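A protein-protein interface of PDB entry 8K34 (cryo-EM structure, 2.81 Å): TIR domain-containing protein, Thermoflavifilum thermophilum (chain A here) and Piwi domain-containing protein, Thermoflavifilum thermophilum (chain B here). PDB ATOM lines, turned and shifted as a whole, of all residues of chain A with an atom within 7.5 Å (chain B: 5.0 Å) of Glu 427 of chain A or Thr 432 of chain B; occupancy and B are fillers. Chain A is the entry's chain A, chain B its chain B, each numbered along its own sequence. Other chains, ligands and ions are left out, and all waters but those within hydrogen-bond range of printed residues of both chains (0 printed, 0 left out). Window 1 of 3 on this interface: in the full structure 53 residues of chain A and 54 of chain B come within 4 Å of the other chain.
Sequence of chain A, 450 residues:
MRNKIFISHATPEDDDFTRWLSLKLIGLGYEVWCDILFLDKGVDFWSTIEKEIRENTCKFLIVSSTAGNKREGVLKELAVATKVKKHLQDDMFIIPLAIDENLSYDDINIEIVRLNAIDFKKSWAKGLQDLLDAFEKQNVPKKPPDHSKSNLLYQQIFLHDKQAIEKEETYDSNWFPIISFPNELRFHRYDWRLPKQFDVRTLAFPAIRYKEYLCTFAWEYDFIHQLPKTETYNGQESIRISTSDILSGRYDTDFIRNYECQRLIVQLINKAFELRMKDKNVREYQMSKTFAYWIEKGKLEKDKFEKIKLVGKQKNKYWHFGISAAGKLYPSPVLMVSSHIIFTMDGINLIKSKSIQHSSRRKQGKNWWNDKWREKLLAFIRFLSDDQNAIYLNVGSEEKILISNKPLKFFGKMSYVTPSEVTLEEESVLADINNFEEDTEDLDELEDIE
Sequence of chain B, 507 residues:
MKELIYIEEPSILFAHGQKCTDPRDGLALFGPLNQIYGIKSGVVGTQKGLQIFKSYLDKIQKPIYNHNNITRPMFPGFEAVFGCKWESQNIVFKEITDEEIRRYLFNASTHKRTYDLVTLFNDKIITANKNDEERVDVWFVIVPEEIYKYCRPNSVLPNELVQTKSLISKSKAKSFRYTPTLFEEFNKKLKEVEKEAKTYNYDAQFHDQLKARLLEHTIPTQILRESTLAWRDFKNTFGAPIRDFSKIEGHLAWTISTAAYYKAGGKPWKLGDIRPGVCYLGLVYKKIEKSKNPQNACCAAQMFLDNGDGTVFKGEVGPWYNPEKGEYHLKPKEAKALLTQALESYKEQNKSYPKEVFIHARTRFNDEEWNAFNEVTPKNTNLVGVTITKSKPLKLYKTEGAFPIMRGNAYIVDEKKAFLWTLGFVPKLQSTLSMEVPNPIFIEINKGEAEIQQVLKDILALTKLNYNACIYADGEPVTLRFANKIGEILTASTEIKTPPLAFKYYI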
ATOM      1  N   LYS A 366     -24.784  17.277  -4.330  1.00  0.00           N
ATOM      2  CA  LYS A 366     -24.539  18.010  -5.562  1.00  0.00           C
ATOM      3  C   LYS A 366     -25.606  19.081  -5.771  1.00  0.00           C
ATOM      4  O   LYS A 366     -26.711  19.001  -5.227  1.00  0.00           O
ATOM      5  CB  LYS A 366     -24.508  17.037  -6.734  1.00  0.00           C
ATOM      6  CG  LYS A 366     -23.799  15.741  -6.379  1.00  0.00           C
ATOM      7  CD  LYS A 366     -23.839  14.750  -7.515  1.00  0.00           C
ATOM      8  CE  LYS A 366     -25.158  14.003  -7.507  1.00  0.00           C
ATOM      9  NZ  LYS A 366     -25.072  12.692  -8.205  1.00  0.00           N
ATOM     10  N   TRP A 369     -23.222  24.434  -3.264  1.00  0.00           N
ATOM     11  CA  TRP A 369     -21.870  24.976  -3.231  1.00  0.00           C
ATOM     12  C   TRP A 369     -21.693  25.949  -2.065  1.00  0.00           C
ATOM     13  O   TRP A 369     -22.523  26.024  -1.156  1.00  0.00           O
ATOM     14  CB  TRP A 369     -21.482  25.650  -4.552  1.00  0.00           C
ATOM     15  CG  TRP A 369     -20.775  24.754  -5.547  1.00  0.00           C
ATOM     16  CD1 TRP A 369     -19.489  24.903  -5.982  1.00  0.00           C
ATOM     17  CD2 TRP A 369     -21.315  23.645  -6.284  1.00  0.00           C
ATOM     18  NE1 TRP A 369     -19.178  23.931  -6.895  1.00  0.00           N
ATOM     19  CE2 TRP A 369     -20.283  23.150  -7.106  1.00  0.00           C
ATOM     20  CE3 TRP A 369     -22.559  23.014  -6.318  1.00  0.00           C
ATOM     21  CZ2 TRP A 369     -20.458  22.056  -7.947  1.00  0.00           C
ATOM     22  CZ3 TRP A 369     -22.725  21.923  -7.150  1.00  0.00           C
ATOM     23  CH2 TRP A 369     -21.685  21.458  -7.954  1.00  0.00           C
ATOM     24  N   TYR A 416      -9.217  34.225  -6.054  1.00  0.00           N
ATOM     25  CA  TYR A 416      -9.300  34.111  -7.502  1.00  0.00           C
ATOM     26  C   TYR A 416     -10.239  35.177  -8.047  1.00  0.00           C
ATOM     27  O   TYR A 416     -11.122  35.659  -7.329  1.00  0.00           O
ATOM     28  CB  TYR A 416      -9.794  32.722  -7.900  1.00  0.00           C
ATOM     29  CG  TYR A 416     -10.875  32.162  -7.002  1.00  0.00           C
ATOM     30  CD1 TYR A 416     -10.580  31.674  -5.738  1.00  0.00           C
ATOM     31  CD2 TYR A 416     -12.197  32.140  -7.414  1.00  0.00           C
ATOM     32  CE1 TYR A 416     -11.564  31.173  -4.920  1.00  0.00           C
ATOM     33  CE2 TYR A 416     -13.187  31.637  -6.601  1.00  0.00           C
ATOM     34  CZ  TYR A 416     -12.864  31.155  -5.355  1.00  0.00           C
ATOM     35  OH  TYR A 416     -13.841  30.653  -4.531  1.00  0.00           O
ATOM     36  N   GLU A 421     -20.419  32.154 -13.324  1.00  0.00           N
ATOM     37  CA  GLU A 421     -21.116  31.077 -12.632  1.00  0.00           C
ATOM     38  C   GLU A 421     -21.587  29.994 -13.592  1.00  0.00           C
ATOM     39  O   GLU A 421     -21.894  28.884 -13.150  1.00  0.00           O
ATOM     40  CB  GLU A 421     -22.297  31.642 -11.839  1.00  0.00           C
ATOM     41  CG  GLU A 421     -22.719  30.792 -10.645  1.00  0.00           C
ATOM     42  CD  GLU A 421     -23.783  29.768 -10.991  1.00  0.00           C
ATOM     43  OE1 GLU A 421     -24.097  28.922 -10.127  1.00  0.00           O
ATOM     44  OE2 GLU A 421     -24.314  29.816 -12.120  1.00  0.00           O
ATOM     45  N   VAL A 422     -21.643  30.287 -14.893  1.00  0.00           N
ATOM     46  CA  VAL A 422     -22.011  29.258 -15.862  1.00  0.00           C
ATOM     47  C   VAL A 422     -20.942  28.173 -15.917  1.00  0.00           C
ATOM     48  O   VAL A 422     -21.233  27.009 -16.211  1.00  0.00           O
ATOM     49  CB  VAL A 422     -22.265  29.884 -17.247  1.00  0.00           C
ATOM     50  CG1 VAL A 422     -23.482  30.795 -17.197  1.00  0.00           C
ATOM     51  CG2 VAL A 422     -21.047  30.647 -17.726  1.00  0.00           C
ATOM     52  N   THR A 423     -19.689  28.532 -15.626  1.00  0.00           N
ATOM     53  CA  THR A 423     -18.648  27.517 -15.490  1.00  0.00           C
ATOM     54  C   THR A 423     -18.953  26.580 -14.327  1.00  0.00           C
ATOM     55  O   THR A 423     -18.802  25.356 -14.440  1.00  0.00           O
ATOM     56  CB  THR A 423     -17.283  28.183 -15.303  1.00  0.00           C
ATOM     57  OG1 THR A 423     -16.867  28.776 -16.540  1.00  0.00           O
ATOM     58  CG2 THR A 423     -16.241  27.165 -14.862  1.00  0.00           C
ATOM     59  N   LEU A 424     -19.403  27.135 -13.200  1.00  0.00           N
ATOM     60  CA  LEU A 424     -19.776  26.289 -12.072  1.00  0.00           C
ATOM     61  C   LEU A 424     -21.047  25.505 -12.366  1.00  0.00           C
ATOM     62  O   LEU A 424     -21.262  24.430 -11.801  1.00  0.00           O
ATOM     63  CB  LEU A 424     -19.941  27.128 -10.808  1.00  0.00           C
ATOM     64  CG  LEU A 424     -19.841  26.307  -9.524  1.00  0.00           C
ATOM     65  CD1 LEU A 424     -18.391  25.968  -9.219  1.00  0.00           C
ATOM     66  CD2 LEU A 424     -20.472  27.064  -8.375  1.00  0.00           C
ATOM     67  N   GLU A 425     -21.896  26.013 -13.260  1.00  0.00           N
ATOM     68  CA  GLU A 425     -23.066  25.244 -13.675  1.00  0.00           C
ATOM     69  C   GLU A 425     -22.653  24.067 -14.549  1.00  0.00           C
ATOM     70  O   GLU A 425     -23.231  22.977 -14.463  1.00  0.00           O
ATOM     71  CB  GLU A 425     -24.058  26.146 -14.409  1.00  0.00           C
ATOM     72  CG  GLU A 425     -25.437  25.531 -14.566  1.00  0.00           C
ATOM     73  CD  GLU A 425     -25.934  24.891 -13.284  1.00  0.00           C
ATOM     74  OE1 GLU A 425     -26.310  25.635 -12.355  1.00  0.00           O
ATOM     75  OE2 GLU A 425     -25.944  23.645 -13.205  1.00  0.00           O
ATOM     76  N   GLU A 426     -21.658  24.281 -15.413  1.00  0.00           N
ATOM     77  CA  GLU A 426     -21.039  23.174 -16.135  1.00  0.00           C
ATOM     78  C   GLU A 426     -20.502  22.137 -15.161  1.00  0.00           C
ATOM     79  O   GLU A 426     -20.759  20.936 -15.304  1.00  0.00           O
ATOM     80  CB  GLU A 426     -19.915  23.693 -17.034  1.00  0.00           C
ATOM     81  CG  GLU A 426     -20.360  24.632 -18.142  1.00  0.00           C
ATOM     82  CD  GLU A 426     -19.611  24.395 -19.439  1.00  0.00           C
ATOM     83  OE1 GLU A 426     -19.832  25.156 -20.404  1.00  0.00           O
ATOM     84  OE2 GLU A 426     -18.796  23.449 -19.494  1.00  0.00           O
ATOM     85  N   GLU A 427     -19.740  22.592 -14.161  1.00  0.00           N
ATOM     86  CA  GLU A 427     -19.292  21.693 -13.102  1.00  0.00           C
ATOM     87  C   GLU A 427     -20.455  20.927 -12.492  1.00  0.00           C
ATOM     88  O   GLU A 427     -20.403  19.701 -12.378  1.00  0.00           O
ATOM     89  CB  GLU A 427     -18.569  22.464 -12.001  1.00  0.00           C
ATOM     90  CG  GLU A 427     -17.081  22.600 -12.169  1.00  0.00           C
ATOM     91  CD  GLU A 427     -16.366  22.370 -10.852  1.00  0.00           C
ATOM     92  OE1 GLU A 427     -15.376  23.069 -10.578  1.00  0.00           O
ATOM     93  OE2 GLU A 427     -16.803  21.484 -10.088  1.00  0.00           O
ATOM     94  N   SER A 428     -21.510  21.639 -12.100  1.00  0.00           N
ATOM     95  CA  SER A 428     -22.629  21.009 -11.413  1.00  0.00           C
ATOM     96  C   SER A 428     -23.252  19.920 -12.273  1.00  0.00           C
ATOM     97  O   SER A 428     -23.383  18.776 -11.832  1.00  0.00           O
ATOM     98  CB  SER A 428     -23.667  22.066 -11.035  1.00  0.00           C
ATOM     99  OG  SER A 428     -23.042  23.221 -10.502  1.00  0.00           O
ATOM    100  N   VAL A 429     -23.601  20.246 -13.518  1.00  0.00           N
ATOM    101  CA  VAL A 429     -24.284  19.278 -14.372  1.00  0.00           C
ATOM    102  C   VAL A 429     -23.377  18.091 -14.687  1.00  0.00           C
ATOM    103  O   VAL A 429     -23.779  16.927 -14.534  1.00  0.00           O
ATOM    104  CB  VAL A 429     -24.788  19.963 -15.655  1.00  0.00           C
ATOM    105  CG1 VAL A 429     -25.444  18.946 -16.577  1.00  0.00           C
ATOM    106  CG2 VAL A 429     -25.761  21.080 -15.310  1.00  0.00           C
ATOM    107  N   LEU A 430     -22.141  18.358 -15.125  1.00  0.00           N
ATOM    108  CA  LEU A 430     -21.265  17.266 -15.535  1.00  0.00           C
ATOM    109  C   LEU A 430     -20.901  16.372 -14.355  1.00  0.00           C
ATOM    110  O   LEU A 430     -20.961  15.143 -14.461  1.00  0.00           O
ATOM    111  CB  LEU A 430     -20.002  17.817 -16.201  1.00  0.00           C
ATOM    112  CG  LEU A 430     -20.129  18.756 -17.409  1.00  0.00           C
ATOM    113  CD1 LEU A 430     -18.878  18.694 -18.274  1.00  0.00           C
ATOM    114  CD2 LEU A 430     -21.373  18.466 -18.241  1.00  0.00           C
ATOM    115  N   ALA A 431     -20.531  16.969 -13.219  1.00  0.00           N
ATOM    116  CA  ALA A 431     -20.169  16.184 -12.047  1.00  0.00           C
ATOM    117  C   ALA A 431     -21.380  15.467 -11.464  1.00  0.00           C
ATOM    118  O   ALA A 431     -21.246  14.381 -10.894  1.00  0.00           O
ATOM    119  CB  ALA A 431     -19.520  17.088 -11.003  1.00  0.00           C
ATOM    120  N   ASP A 432     -22.570  16.057 -11.595  1.00  0.00           N
ATOM    121  CA  ASP A 432     -23.790  15.377 -11.182  1.00  0.00           C
ATOM    122  C   ASP A 432     -24.010  14.117 -12.005  1.00  0.00           C
ATOM    123  O   ASP A 432     -24.310  13.048 -11.455  1.00  0.00           O
ATOM    124  CB  ASP A 432     -24.972  16.339 -11.322  1.00  0.00           C
ATOM    125  CG  ASP A 432     -26.296  15.707 -10.959  1.00  0.00           C
ATOM    126  OD1 ASP A 432     -26.298  14.730 -10.190  1.00  0.00           O
ATOM    127  OD2 ASP A 432     -27.339  16.192 -11.445  1.00  0.00           O
ATOM    128  N   ILE A 433     -23.836  14.217 -13.323  1.00  0.00           N
ATOM    129  CA  ILE A 433     -23.956  13.036 -14.174  1.00  0.00           C
ATOM    130  C   ILE A 433     -22.889  12.009 -13.813  1.00  0.00           C
ATOM    131  O   ILE A 433     -23.162  10.804 -13.740  1.00  0.00           O
ATOM    132  CB  ILE A 433     -23.882  13.438 -15.659  1.00  0.00           C
ATOM    133  CG1 ILE A 433     -25.192  14.095 -16.096  1.00  0.00           C
ATOM    134  CG2 ILE A 433     -23.575  12.225 -16.525  1.00  0.00           C
ATOM    135  CD1 ILE A 433     -26.416  13.235 -15.862  1.00  0.00           C
ATOM    136  N   ASN A 434     -21.659  12.469 -13.573  1.00  0.00           N
ATOM    137  CA  ASN A 434     -20.573  11.551 -13.240  1.00  0.00           C
ATOM    138  C   ASN A 434     -20.839  10.822 -11.929  1.00  0.00           C
ATOM    139  O   ASN A 434     -20.572   9.619 -11.815  1.00  0.00           O
ATOM    140  CB  ASN A 434     -19.245  12.306 -13.175  1.00  0.00           C
ATOM    141  CG  ASN A 434     -18.886  12.965 -14.490  1.00  0.00           C
ATOM    142  OD1 ASN A 434     -18.359  14.077 -14.519  1.00  0.00           O
ATOM    143  ND2 ASN A 434     -19.177  12.283 -15.591  1.00  0.00           N
ATOM    144  N   PRO B 404     -15.995  27.841  -3.823  1.00  0.00           N
ATOM    145  CA  PRO B 404     -15.409  27.625  -2.493  1.00  0.00           C
ATOM    146  C   PRO B 404     -14.043  28.264  -2.322  1.00  0.00           C
ATOM    147  O   PRO B 404     -13.496  28.843  -3.265  1.00  0.00           O
ATOM    148  CB  PRO B 404     -15.320  26.098  -2.397  1.00  0.00           C
ATOM    149  CG  PRO B 404     -15.341  25.618  -3.800  1.00  0.00           C
ATOM    150  CD  PRO B 404     -16.193  26.580  -4.556  1.00  0.00           C
ATOM    151  N   GLY B 424     -10.954  22.002  -3.404  1.00  0.00           N
ATOM    152  CA  GLY B 424     -11.600  23.270  -3.648  1.00  0.00           C
ATOM    153  C   GLY B 424     -11.269  23.851  -5.007  1.00  0.00           C
ATOM    154  O   GLY B 424     -10.750  23.186  -5.906  1.00  0.00           O
ATOM    155  N   PHE B 425     -11.578  25.135  -5.145  1.00  0.00           N
ATOM    156  CA  PHE B 425     -11.422  25.835  -6.411  1.00  0.00           C
ATOM    157  C   PHE B 425      -9.945  26.079  -6.687  1.00  0.00           C
ATOM    158  O   PHE B 425      -9.195  26.457  -5.785  1.00  0.00           O
ATOM    159  CB  PHE B 425     -12.196  27.150  -6.380  1.00  0.00           C
ATOM    160  CG  PHE B 425     -12.214  27.882  -7.690  1.00  0.00           C
ATOM    161  CD1 PHE B 425     -13.259  27.708  -8.578  1.00  0.00           C
ATOM    162  CD2 PHE B 425     -11.201  28.766  -8.022  1.00  0.00           C
ATOM    163  CE1 PHE B 425     -13.285  28.381  -9.776  1.00  0.00           C
ATOM    164  CE2 PHE B 425     -11.222  29.442  -9.220  1.00  0.00           C
ATOM    165  CZ  PHE B 425     -12.267  29.251 -10.095  1.00  0.00           C
ATOM    166  N   VAL B 426      -9.521  25.841  -7.916  1.00  0.00           N
ATOM    167  CA  VAL B 426      -8.174  26.182  -8.367  1.00  0.00           C
ATOM    168  C   VAL B 426      -8.291  27.153  -9.536  1.00  0.00           C
ATOM    169  O   VAL B 426      -9.059  26.886 -10.471  1.00  0.00           O
ATOM    170  CB  VAL B 426      -7.368  24.932  -8.759  1.00  0.00           C
ATOM    171  CG1 VAL B 426      -8.188  24.012  -9.637  1.00  0.00           C
ATOM    172  CG2 VAL B 426      -6.098  25.342  -9.470  1.00  0.00           C
ATOM    173  N   GLN B 430     -10.066  26.930 -13.240  1.00  0.00           N
ATOM    174  CA  GLN B 430     -11.310  27.658 -12.999  1.00  0.00           C
ATOM    175  C   GLN B 430     -12.399  26.690 -12.552  1.00  0.00           C
ATOM    176  O   GLN B 430     -13.550  26.761 -12.989  1.00  0.00           O
ATOM    177  CB  GLN B 430     -11.747  28.452 -14.232  1.00  0.00           C
ATOM    178  CG  GLN B 430     -10.696  29.409 -14.766  1.00  0.00           C
ATOM    179  CD  GLN B 430     -10.512  30.649 -13.910  1.00  0.00           C
ATOM    180  OE1 GLN B 430     -11.053  30.750 -12.810  1.00  0.00           O
ATOM    181  NE2 GLN B 430      -9.742  31.604 -14.416  1.00  0.00           N
ATOM    182  N   SER B 431     -12.022  25.767 -11.676  1.00  0.00           N
ATOM    183  CA  SER B 431     -12.863  24.634 -11.330  1.00  0.00           C
ATOM    184  C   SER B 431     -12.494  24.168  -9.928  1.00  0.00           C
ATOM    185  O   SER B 431     -11.545  24.673  -9.318  1.00  0.00           O
ATOM    186  CB  SER B 431     -12.709  23.514 -12.363  1.00  0.00           C
ATOM    187  OG  SER B 431     -13.820  22.638 -12.340  1.00  0.00           O
ATOM    188  N   THR B 432     -13.237  23.189  -9.423  1.00  0.00           N
ATOM    189  CA  THR B 432     -13.055  22.667  -8.079  1.00  0.00           C
ATOM    190  C   THR B 432     -12.748  21.179  -8.141  1.00  0.00           C
ATOM    191  O   THR B 432     -13.397  20.430  -8.877  1.00  0.00           O
ATOM    192  CB  THR B 432     -14.304  22.891  -7.218  1.00  0.00           C
ATOM    193  OG1 THR B 432     -15.409  22.171  -7.779  1.00  0.00           O
ATOM    194  CG2 THR B 432     -14.653  24.366  -7.157  1.00  0.00           C
ATOM    195  N   LEU B 433     -11.750  20.753  -7.365  1.00  0.00           N
ATOM    196  CA  LEU B 433     -11.478  19.329  -7.228  1.00  0.00           C
ATOM    197  C   LEU B 433     -12.510  18.652  -6.336  1.00  0.00           C
ATOM    198  O   LEU B 433     -12.923  17.519  -6.606  1.00  0.00           O
ATOM    199  CB  LEU B 433     -10.069  19.119  -6.673  1.00  0.00           C
ATOM    200  CG  LEU B 433      -8.976  20.011  -7.265  1.00  0.00           C
ATOM    201  CD1 LEU B 433      -7.734  19.962  -6.402  1.00  0.00           C
ATOM    202  CD2 LEU B 433      -8.648  19.584  -8.682  1.00  0.00           C
ATOM    203  N   SER B 434     -12.943  19.335  -5.279  1.00  0.00           N
ATOM    204  CA  SER B 434     -13.902  18.801  -4.326  1.00  0.00           C
ATOM    205  C   SER B 434     -15.321  18.923  -4.865  1.00  0.00           C
ATOM    206  O   SER B 434     -15.629  19.789  -5.686  1.00  0.00           O
ATOM    207  CB  SER B 434     -13.794  19.532  -2.989  1.00  0.00           C
ATOM    208  OG  SER B 434     -13.948  20.929  -3.167  1.00  0.00           O
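N of Thr 432 of chain B sits at hydrogen-bond distance from OE1 of Glu 427 of chain A (2.4 Å).
The side-chain hydroxyl of Tyr 416 of chain A sits close to the backbone carbonyl oxygen of Pro 404 of chain B (2.2 Å).
The side-chain hydroxyl of Ser 431 of chain B sits close to the side-chain carboxylate of Glu 427 of chain A (2.4 Å).
The backbone carbonyl oxygen of Ser 431 of chain B lies within hydrogen-bond range of the backbone NH of Val 426 of chain B (2.7 Å).
OG1 of Thr 432 of chain B lies within hydrogen-bond range of O of Ser 434 of chain B (3.2 Å).
CD of Pro 404 of chain B touches CD1 of Trp 369 of chain A, at 3.96 Å.
Tyr 416 of chain A touches Phe 425 of chain B.
CG2 of Thr 423 of chain A touches O of Gln 430 of chain B, at 3.3 Å.
Glu 427 of chain A touches just these residues of chain B: Ser 431 (2.4 Å) and Thr 432 (2.4 Å).
Printed residues of chain A within 4 Å of Gln 430 of chain B: Thr 423 (3.3 Å).
Of the printed residues of chain A, Ser 431 of chain B touches Glu 427 (2.4 Å).
Of the printed residues of chain A, Phe 425 of chain B touches Tyr 416 (3.4 Å).
Of the printed residues of chain B, Thr 423 of chain A touches Gln 430 (3.3 Å).
Of the printed residues of chain B, Tyr 416 of chain A touches Pro 404 and Phe 425.
Val 422 of chain A touches none of the printed residues of chain B.
Leu 433 of chain B touches none of the printed residues of chain A.
The nearest printed residue of chain B that does not touch Trp 369 of chain A is Thr 432 of chain B (4.3 Å).
Printed residues of chain B that touch a printed residue of chain A: Pro 404, Phe 425, Gln 430, Ser 431 and Thr 432.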
